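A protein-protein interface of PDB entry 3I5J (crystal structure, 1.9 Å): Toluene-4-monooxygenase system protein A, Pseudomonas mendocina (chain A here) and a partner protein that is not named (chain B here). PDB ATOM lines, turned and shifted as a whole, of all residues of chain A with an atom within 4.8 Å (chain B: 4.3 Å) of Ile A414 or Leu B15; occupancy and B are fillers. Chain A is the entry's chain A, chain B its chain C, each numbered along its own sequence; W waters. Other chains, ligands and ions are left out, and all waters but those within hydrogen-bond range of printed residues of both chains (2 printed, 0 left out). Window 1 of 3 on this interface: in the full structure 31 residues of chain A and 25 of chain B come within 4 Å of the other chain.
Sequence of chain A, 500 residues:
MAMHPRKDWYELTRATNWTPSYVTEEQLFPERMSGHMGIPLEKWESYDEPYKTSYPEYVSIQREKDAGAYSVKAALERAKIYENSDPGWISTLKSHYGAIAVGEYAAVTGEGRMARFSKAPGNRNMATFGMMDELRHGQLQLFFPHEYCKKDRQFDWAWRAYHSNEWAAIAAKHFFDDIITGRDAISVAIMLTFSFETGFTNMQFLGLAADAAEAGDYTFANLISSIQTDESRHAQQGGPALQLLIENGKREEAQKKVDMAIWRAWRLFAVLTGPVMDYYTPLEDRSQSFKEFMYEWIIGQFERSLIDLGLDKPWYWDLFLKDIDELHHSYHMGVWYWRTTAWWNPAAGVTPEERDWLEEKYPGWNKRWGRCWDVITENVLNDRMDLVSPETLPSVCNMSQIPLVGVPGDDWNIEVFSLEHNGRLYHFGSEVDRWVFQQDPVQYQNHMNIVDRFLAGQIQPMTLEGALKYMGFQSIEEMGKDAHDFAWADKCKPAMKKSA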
ATOM      1  N   TRP A 338     -26.497 -13.104   4.200  1.00  0.00           N
ATOM      2  CA  TRP A 338     -25.214 -12.900   4.881  1.00  0.00           C
ATOM      3  C   TRP A 338     -25.334 -13.386   6.364  1.00  0.00           C
ATOM      4  O   TRP A 338     -24.691 -12.812   7.256  1.00  0.00           O
ATOM      5  CB  TRP A 338     -24.753 -11.424   4.740  1.00  0.00           C
ATOM      6  CG  TRP A 338     -23.999 -11.150   3.387  1.00  0.00           C
ATOM      7  CD1 TRP A 338     -22.631 -11.205   3.164  1.00  0.00           C
ATOM      8  CD2 TRP A 338     -24.599 -10.879   2.106  1.00  0.00           C
ATOM      9  NE1 TRP A 338     -22.349 -10.944   1.842  1.00  0.00           N
ATOM     10  CE2 TRP A 338     -23.529 -10.747   1.162  1.00  0.00           C
ATOM     11  CE3 TRP A 338     -25.935 -10.716   1.664  1.00  0.00           C
ATOM     12  CZ2 TRP A 338     -23.743 -10.467  -0.185  1.00  0.00           C
ATOM     13  CZ3 TRP A 338     -26.147 -10.430   0.304  1.00  0.00           C
ATOM     14  CH2 TRP A 338     -25.048 -10.305  -0.606  1.00  0.00           C
ATOM     15  N   PRO A 394     -21.877  -7.000   0.793  1.00  0.00           N
ATOM     16  CA  PRO A 394     -22.804  -5.979   0.322  1.00  0.00           C
ATOM     17  C   PRO A 394     -22.163  -4.623   0.359  1.00  0.00           C
ATOM     18  O   PRO A 394     -21.212  -4.422   1.141  1.00  0.00           O
ATOM     19  CB  PRO A 394     -23.901  -5.961   1.360  1.00  0.00           C
ATOM     20  CG  PRO A 394     -23.535  -7.002   2.391  1.00  0.00           C
ATOM     21  CD  PRO A 394     -22.232  -7.588   2.106  1.00  0.00           C
ATOM     22  N   LEU A 404     -27.093  -1.374   1.006  1.00  0.00           N
ATOM     23  CA  LEU A 404     -27.865  -0.656   0.034  1.00  0.00           C
ATOM     24  C   LEU A 404     -28.792  -1.600  -0.732  1.00  0.00           C
ATOM     25  O   LEU A 404     -28.343  -2.478  -1.456  1.00  0.00           O
ATOM     26  CB  LEU A 404     -26.915   0.024  -0.940  1.00  0.00           C
ATOM     27  CG  LEU A 404     -25.906   1.037  -0.399  1.00  0.00           C
ATOM     28  CD1 LEU A 404     -24.810   1.386  -1.388  1.00  0.00           C
ATOM     29  CD2 LEU A 404     -26.686   2.339   0.087  1.00  0.00           C
ATOM     30  N   VAL A 405     -30.093  -1.353  -0.653  1.00  0.00           N
ATOM     31  CA  VAL A 405     -31.081  -2.297  -1.167  1.00  0.00           C
ATOM     32  C   VAL A 405     -32.101  -1.587  -2.049  1.00  0.00           C
ATOM     33  O   VAL A 405     -32.145  -0.353  -2.088  1.00  0.00           O
ATOM     34  CB  VAL A 405     -31.757  -3.067   0.029  1.00  0.00           C
ATOM     35  CG1 VAL A 405     -30.745  -3.965   0.787  1.00  0.00           C
ATOM     36  CG2 VAL A 405     -32.547  -2.082   0.985  1.00  0.00           C
ATOM     37  N   GLY A 406     -32.897  -2.365  -2.774  1.00  0.00           N
ATOM     38  CA  GLY A 406     -34.012  -1.838  -3.533  1.00  0.00           C
ATOM     39  C   GLY A 406     -35.112  -2.880  -3.612  1.00  0.00           C
ATOM     40  O   GLY A 406     -35.088  -3.906  -2.863  1.00  0.00           O
ATOM     41  N   TRP A 412     -38.277  -4.334 -10.651  1.00  0.00           N
ATOM     42  CA  TRP A 412     -36.990  -3.987 -10.063  1.00  0.00           C
ATOM     43  C   TRP A 412     -36.725  -2.516 -10.012  1.00  0.00           C
ATOM     44  O   TRP A 412     -36.760  -1.849 -11.025  1.00  0.00           O
ATOM     45  CB  TRP A 412     -35.884  -4.620 -10.903  1.00  0.00           C
ATOM     46  CG  TRP A 412     -34.489  -4.345 -10.464  1.00  0.00           C
ATOM     47  CD1 TRP A 412     -33.910  -4.675  -9.253  1.00  0.00           C
ATOM     48  CD2 TRP A 412     -33.456  -3.693 -11.229  1.00  0.00           C
ATOM     49  NE1 TRP A 412     -32.580  -4.276  -9.243  1.00  0.00           N
ATOM     50  CE2 TRP A 412     -32.280  -3.671 -10.429  1.00  0.00           C
ATOM     51  CE3 TRP A 412     -33.407  -3.122 -12.516  1.00  0.00           C
ATOM     52  CZ2 TRP A 412     -31.075  -3.117 -10.878  1.00  0.00           C
ATOM     53  CZ3 TRP A 412     -32.193  -2.570 -12.960  1.00  0.00           C
ATOM     54  CH2 TRP A 412     -31.043  -2.580 -12.145  1.00  0.00           C
ATOM     55  N   ASN A 413     -36.492  -1.995  -8.813  1.00  0.00           N
ATOM     56  CA  ASN A 413     -35.986  -0.646  -8.696  1.00  0.00           C
ATOM     57  C   ASN A 413     -34.996  -0.540  -7.544  1.00  0.00           C
ATOM     58  O   ASN A 413     -35.262  -1.022  -6.441  1.00  0.00           O
ATOM     59  CB  ASN A 413     -37.137   0.372  -8.528  1.00  0.00           C
ATOM     60  CG  ASN A 413     -36.648   1.811  -8.533  1.00  0.00           C
ATOM     61  OD1 ASN A 413     -36.446   2.401  -9.594  1.00  0.00           O
ATOM     62  ND2 ASN A 413     -36.438   2.375  -7.342  1.00  0.00           N
ATOM     63  N   ILE A 414     -33.848   0.074  -7.797  1.00  0.00           N
ATOM     64  CA  ILE A 414     -32.899   0.318  -6.717  1.00  0.00           C
ATOM     65  C   ILE A 414     -32.196   1.647  -6.941  1.00  0.00           C
ATOM     66  O   ILE A 414     -31.900   2.026  -8.101  1.00  0.00           O
ATOM     67  CB  ILE A 414     -31.874  -0.815  -6.600  1.00  0.00           C
ATOM     68  CG1 ILE A 414     -30.879  -0.571  -5.447  1.00  0.00           C
ATOM     69  CG2 ILE A 414     -31.092  -1.058  -7.935  1.00  0.00           C
ATOM     70  CD1 ILE A 414     -30.156  -1.957  -5.054  1.00  0.00           C
ATOM     71  N   GLU A 415     -31.925   2.376  -5.845  1.00  0.00           N
ATOM     72  CA  GLU A 415     -31.257   3.652  -6.066  1.00  0.00           C
ATOM     73  C   GLU A 415     -30.241   3.954  -4.953  1.00  0.00           C
ATOM     74  O   GLU A 415     -30.555   3.829  -3.769  1.00  0.00           O
ATOM     75  CB  GLU A 415     -32.256   4.806  -6.173  1.00  0.00           C
ATOM     76  CG  GLU A 415     -31.478   6.094  -6.675  1.00  0.00           C
ATOM     77  CD  GLU A 415     -32.379   7.231  -7.127  1.00  0.00           C
ATOM     78  OE1 GLU A 415     -33.629   7.051  -7.194  1.00  0.00           O
ATOM     79  OE2 GLU A 415     -31.810   8.296  -7.443  1.00  0.00           O
ATOM     80  N   VAL A 416     -29.017   4.292  -5.351  1.00  0.00           N
ATOM     81  CA  VAL A 416     -28.000   4.752  -4.409  1.00  0.00           C
ATOM     82  C   VAL A 416     -27.872   6.265  -4.551  1.00  0.00           C
ATOM     83  O   VAL A 416     -27.907   6.763  -5.650  1.00  0.00           O
ATOM     84  CB  VAL A 416     -26.658   4.044  -4.640  1.00  0.00           C
ATOM     85  CG1 VAL A 416     -25.535   4.586  -3.722  1.00  0.00           C
ATOM     86  CG2 VAL A 416     -26.905   2.522  -4.453  1.00  0.00           C
ATOM     87  N   ALA B   8     -22.003  -2.762  -7.553  1.00  0.00           N
ATOM     88  CA  ALA B   8     -22.838  -3.138  -8.701  1.00  0.00           C
ATOM     89  C   ALA B   8     -24.249  -3.603  -8.346  1.00  0.00           C
ATOM     90  O   ALA B   8     -24.468  -4.464  -7.476  1.00  0.00           O
ATOM     91  CB  ALA B   8     -22.081  -4.237  -9.653  1.00  0.00           C
ATOM     92  N   ALA B   9     -25.225  -3.026  -9.022  1.00  0.00           N
ATOM     93  CA  ALA B   9     -26.616  -3.470  -8.854  1.00  0.00           C
ATOM     94  C   ALA B   9     -27.055  -4.363 -10.051  1.00  0.00           C
ATOM     95  O   ALA B   9     -27.116  -3.868 -11.175  1.00  0.00           O
ATOM     96  CB  ALA B   9     -27.524  -2.279  -8.671  1.00  0.00           C
ATOM     97  N   ASP B  13     -32.269  -8.097  -8.898  1.00  0.00           N
ATOM     98  CA  ASP B  13     -31.682  -8.411  -7.625  1.00  0.00           C
ATOM     99  C   ASP B  13     -32.240  -7.386  -6.602  1.00  0.00           C
ATOM    100  O   ASP B  13     -32.868  -6.405  -7.009  1.00  0.00           O
ATOM    101  CB  ASP B  13     -30.160  -8.384  -7.686  1.00  0.00           C
ATOM    102  CG  ASP B  13     -29.516  -9.227  -6.591  1.00  0.00           C
ATOM    103  OD1 ASP B  13     -30.248  -9.829  -5.708  1.00  0.00           O
ATOM    104  OD2 ASP B  13     -28.256  -9.321  -6.599  1.00  0.00           O
ATOM    105  N   PHE B  14     -31.991  -7.611  -5.316  1.00  0.00           N
ATOM    106  CA  PHE B  14     -32.493  -6.721  -4.283  1.00  0.00           C
ATOM    107  C   PHE B  14     -31.453  -5.804  -3.650  1.00  0.00           C
ATOM    108  O   PHE B  14     -31.833  -5.002  -2.781  1.00  0.00           O
ATOM    109  CB  PHE B  14     -33.103  -7.541  -3.136  1.00  0.00           C
ATOM    110  CG  PHE B  14     -32.066  -8.034  -2.162  1.00  0.00           C
ATOM    111  CD1 PHE B  14     -31.871  -7.379  -0.959  1.00  0.00           C
ATOM    112  CD2 PHE B  14     -31.215  -9.091  -2.512  1.00  0.00           C
ATOM    113  CE1 PHE B  14     -30.898  -7.803  -0.072  1.00  0.00           C
ATOM    114  CE2 PHE B  14     -30.220  -9.544  -1.638  1.00  0.00           C
ATOM    115  CZ  PHE B  14     -30.081  -8.902  -0.390  1.00  0.00           C
ATOM    116  N   LEU B  15     -30.175  -5.956  -4.008  1.00  0.00           N
ATOM    117  CA  LEU B  15     -29.180  -5.074  -3.429  1.00  0.00           C
ATOM    118  C   LEU B  15     -28.043  -4.646  -4.372  1.00  0.00           C
ATOM    119  O   LEU B  15     -27.887  -5.084  -5.554  1.00  0.00           O
ATOM    120  CB  LEU B  15     -28.508  -5.741  -2.242  1.00  0.00           C
ATOM    121  CG  LEU B  15     -27.344  -6.678  -2.539  1.00  0.00           C
ATOM    122  CD1 LEU B  15     -26.673  -7.112  -1.216  1.00  0.00           C
ATOM    123  CD2 LEU B  15     -27.754  -7.916  -3.360  1.00  0.00           C
ATOM    124  N   VAL B  16     -27.229  -3.766  -3.796  1.00  0.00           N
ATOM    125  CA  VAL B  16     -25.984  -3.384  -4.434  1.00  0.00           C
ATOM    126  C   VAL B  16     -24.841  -4.097  -3.763  1.00  0.00           C
ATOM    127  O   VAL B  16     -24.803  -4.179  -2.548  1.00  0.00           O
ATOM    128  CB  VAL B  16     -25.732  -1.822  -4.395  1.00  0.00           C
ATOM    129  CG1 VAL B  16     -24.499  -1.438  -5.223  1.00  0.00           C
ATOM    130  CG2 VAL B  16     -26.980  -1.033  -4.830  1.00  0.00           C
ATOM    131  N   GLN B  17     -23.870  -4.597  -4.536  1.00  0.00           N
ATOM    132  CA  GLN B  17     -22.798  -5.389  -3.978  1.00  0.00           C
ATOM    133  C   GLN B  17     -21.457  -4.877  -4.390  1.00  0.00           C
ATOM    134  O   GLN B  17     -21.315  -4.372  -5.546  1.00  0.00           O
ATOM    135  CB  GLN B  17     -22.891  -6.857  -4.454  1.00  0.00           C
ATOM    136  CG  GLN B  17     -23.979  -7.689  -3.795  1.00  0.00           C
ATOM    137  CD  GLN B  17     -24.031  -9.061  -4.421  1.00  0.00           C
ATOM    138  OE1 GLN B  17     -23.984  -9.180  -5.668  1.00  0.00           O
ATOM    139  NE2 GLN B  17     -24.079 -10.087  -3.623  1.00  0.00           N
ATOM    140  N   ARG B  42     -29.897 -15.115  -6.483  1.00  0.00           N
ATOM    141  CA  ARG B  42     -31.145 -14.404  -6.126  1.00  0.00           C
ATOM    142  C   ARG B  42     -31.943 -13.978  -7.350  1.00  0.00           C
ATOM    143  O   ARG B  42     -33.080 -13.506  -7.192  1.00  0.00           O
ATOM    144  CB  ARG B  42     -30.836 -13.208  -5.186  1.00  0.00           C
ATOM    145  CG  ARG B  42     -30.195 -13.671  -3.849  1.00  0.00           C
ATOM    146  CD  ARG B  42     -29.868 -12.426  -2.997  1.00  0.00           C
ATOM    147  NE  ARG B  42     -29.047 -11.611  -3.855  1.00  0.00           N
ATOM    148  CZ  ARG B  42     -27.754 -11.855  -4.045  1.00  0.00           C
ATOM    149  NH1 ARG B  42     -27.077 -11.128  -4.907  1.00  0.00           N
ATOM    150  NH2 ARG B  42     -27.162 -12.820  -3.373  1.00  0.00           N
ATOM    151  N   HIS B  55     -24.613   3.897 -12.650  1.00  0.00           N
ATOM    152  CA  HIS B  55     -25.856   3.752 -11.941  1.00  0.00           C
ATOM    153  C   HIS B  55     -26.888   4.811 -12.353  1.00  0.00           C
ATOM    154  O   HIS B  55     -26.583   5.996 -12.374  1.00  0.00           O
ATOM    155  CB  HIS B  55     -25.570   3.814 -10.431  1.00  0.00           C
ATOM    156  CG  HIS B  55     -26.766   3.516  -9.573  1.00  0.00           C
ATOM    157  ND1 HIS B  55     -27.185   4.353  -8.554  1.00  0.00           N
ATOM    158  CD2 HIS B  55     -27.648   2.489  -9.601  1.00  0.00           C
ATOM    159  CE1 HIS B  55     -28.256   3.844  -7.977  1.00  0.00           C
ATOM    160  NE2 HIS B  55     -28.542   2.699  -8.572  1.00  0.00           N
ATOM    161  N   ARG B  56     -28.115   4.344 -12.619  1.00  0.00           N
ATOM    162  CA  ARG B  56     -29.288   5.150 -13.046  1.00  0.00           C
ATOM    163  C   ARG B  56     -29.080   5.850 -14.420  1.00  0.00           C
ATOM    164  O   ARG B  56     -29.927   6.639 -14.838  1.00  0.00           O
ATOM    165  CB  ARG B  56     -29.743   6.240 -12.030  1.00  0.00           C
ATOM    166  CG  ARG B  56     -30.050   5.892 -10.487  1.00  0.00           C
ATOM    167  CD  ARG B  56     -31.221   4.944 -10.205  1.00  0.00           C
ATOM    168  NE  ARG B  56     -32.527   5.613 -10.290  1.00  0.00           N
ATOM    169  CZ  ARG B  56     -33.681   4.987 -10.058  1.00  0.00           C
ATOM    170  NH1 ARG B  56     -33.657   3.702  -9.734  1.00  0.00           N
ATOM    171  NH2 ARG B  56     -34.850   5.625 -10.138  1.00  0.00           N
HETATM  172  O   HOH W   1     -32.807   8.161 -10.750  1.00  0.00           O
HETATM  173  O   HOH W   2     -29.802  -4.693  -8.011  1.00  0.00           O
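Water W1 bridges the guanidinium group of Arg B56 (2.6 Å) and the side-chain carboxylate of Glu A415 (3.5 Å). Water W2 lies within hydrogen-bond range of NE1 of Trp A412 and O of Leu B15.
Of the 10 printed residues of chain B, 8 touch a printed residue of chain A. Of the 10 printed residues of chain A, 10 touch a printed residue of chain B. Printed residues of chain A that touch a printed residue of chain B: Trp A338, Pro A394, Leu A404, Val A405, Gly A406, Trp A412, Asn A413, Ile A414, Glu A415 and Val A416. Among the printed residues, Asp or Glu carboxylates within 4 Å of a Lys or Arg side-chain nitrogen of the other chain: Glu A415 with Arg B56.
The backbone NH (N) of Val B16 is in hydrogen-bond range of the backbone carbonyl oxygen (O) of Leu A404 (2.9 Å). The backbone NH (N) of Gly A406 sits at hydrogen-bond distance from the backbone carbonyl oxygen (O) of Phe B14 (2.8 Å). The indole nitrogen of Trp A412 lies close to the backbone carbonyl oxygen of Asp B13, at 3.1 Å. The guanidinium group (NH1) of Arg B56 is in hydrogen-bond range of the side-chain amide oxygen (OD1) of Asn A413 (3.1 Å). NE2 of His B55 lies within hydrogen-bond range of O of Ile A414. O of Ile A414 sits at hydrogen-bond distance from NH1 of Arg B56 (2.9 Å). The side-chain carboxylate (OE1) of Glu A415 lies within salt-bridge range of the guanidinium group (NH2) of Arg B56, at 3.5 Å.
The backbone NH (N) of Ala B8 lies within hydrogen-bond range of the backbone carbonyl oxygen (O) of Gln B17 (2.7 Å). OD2 of Asp B13 lies within salt-bridge range of NH1 of Arg B42 (2.7 Å). The guanidinium group (NH1) of Arg B42 lies close to the side-chain amide nitrogen (NE2) of Gln B17.
Printed residues of chain B within 4 Å of Leu A404: Leu B15 and Val B16. Printed residues of chain B within 4 Å of Val A405: Phe B14 (3.2 Å). Of chain B, only Ala B9 (3.8 Å), Leu B15 (3.5 Å), Val B16 (3.3 Å), His B55 (3.5 Å) and Arg B56 (2.9 Å) come within 4 Å of Ile A414. Ala B8 touches none of the printed residues of chain A. Leu B15 touches four residues of chain A. Of the printed residues of chain A, Val B16 touches Pro A394, Leu A404, Ile A414 and Val A416. The nearest residue of chain B that does not touch Ile A414 is Phe B14 (4.2 Å).
Among the printed residues, pairs that only touch across the chains: Val A416 with His B55, Trp A338 with Gln B17, Val A405 with Phe B14, Ile A414 with Val B16, Leu A404 with Leu B15, Ile A414 with Leu B15, Glu A415 with His B55, Val A416 with Val B16, Trp A338 with Leu B15, Ile A414 with Ala B9, Pro A394 with Val B16 and Pro A394 with Leu B15.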
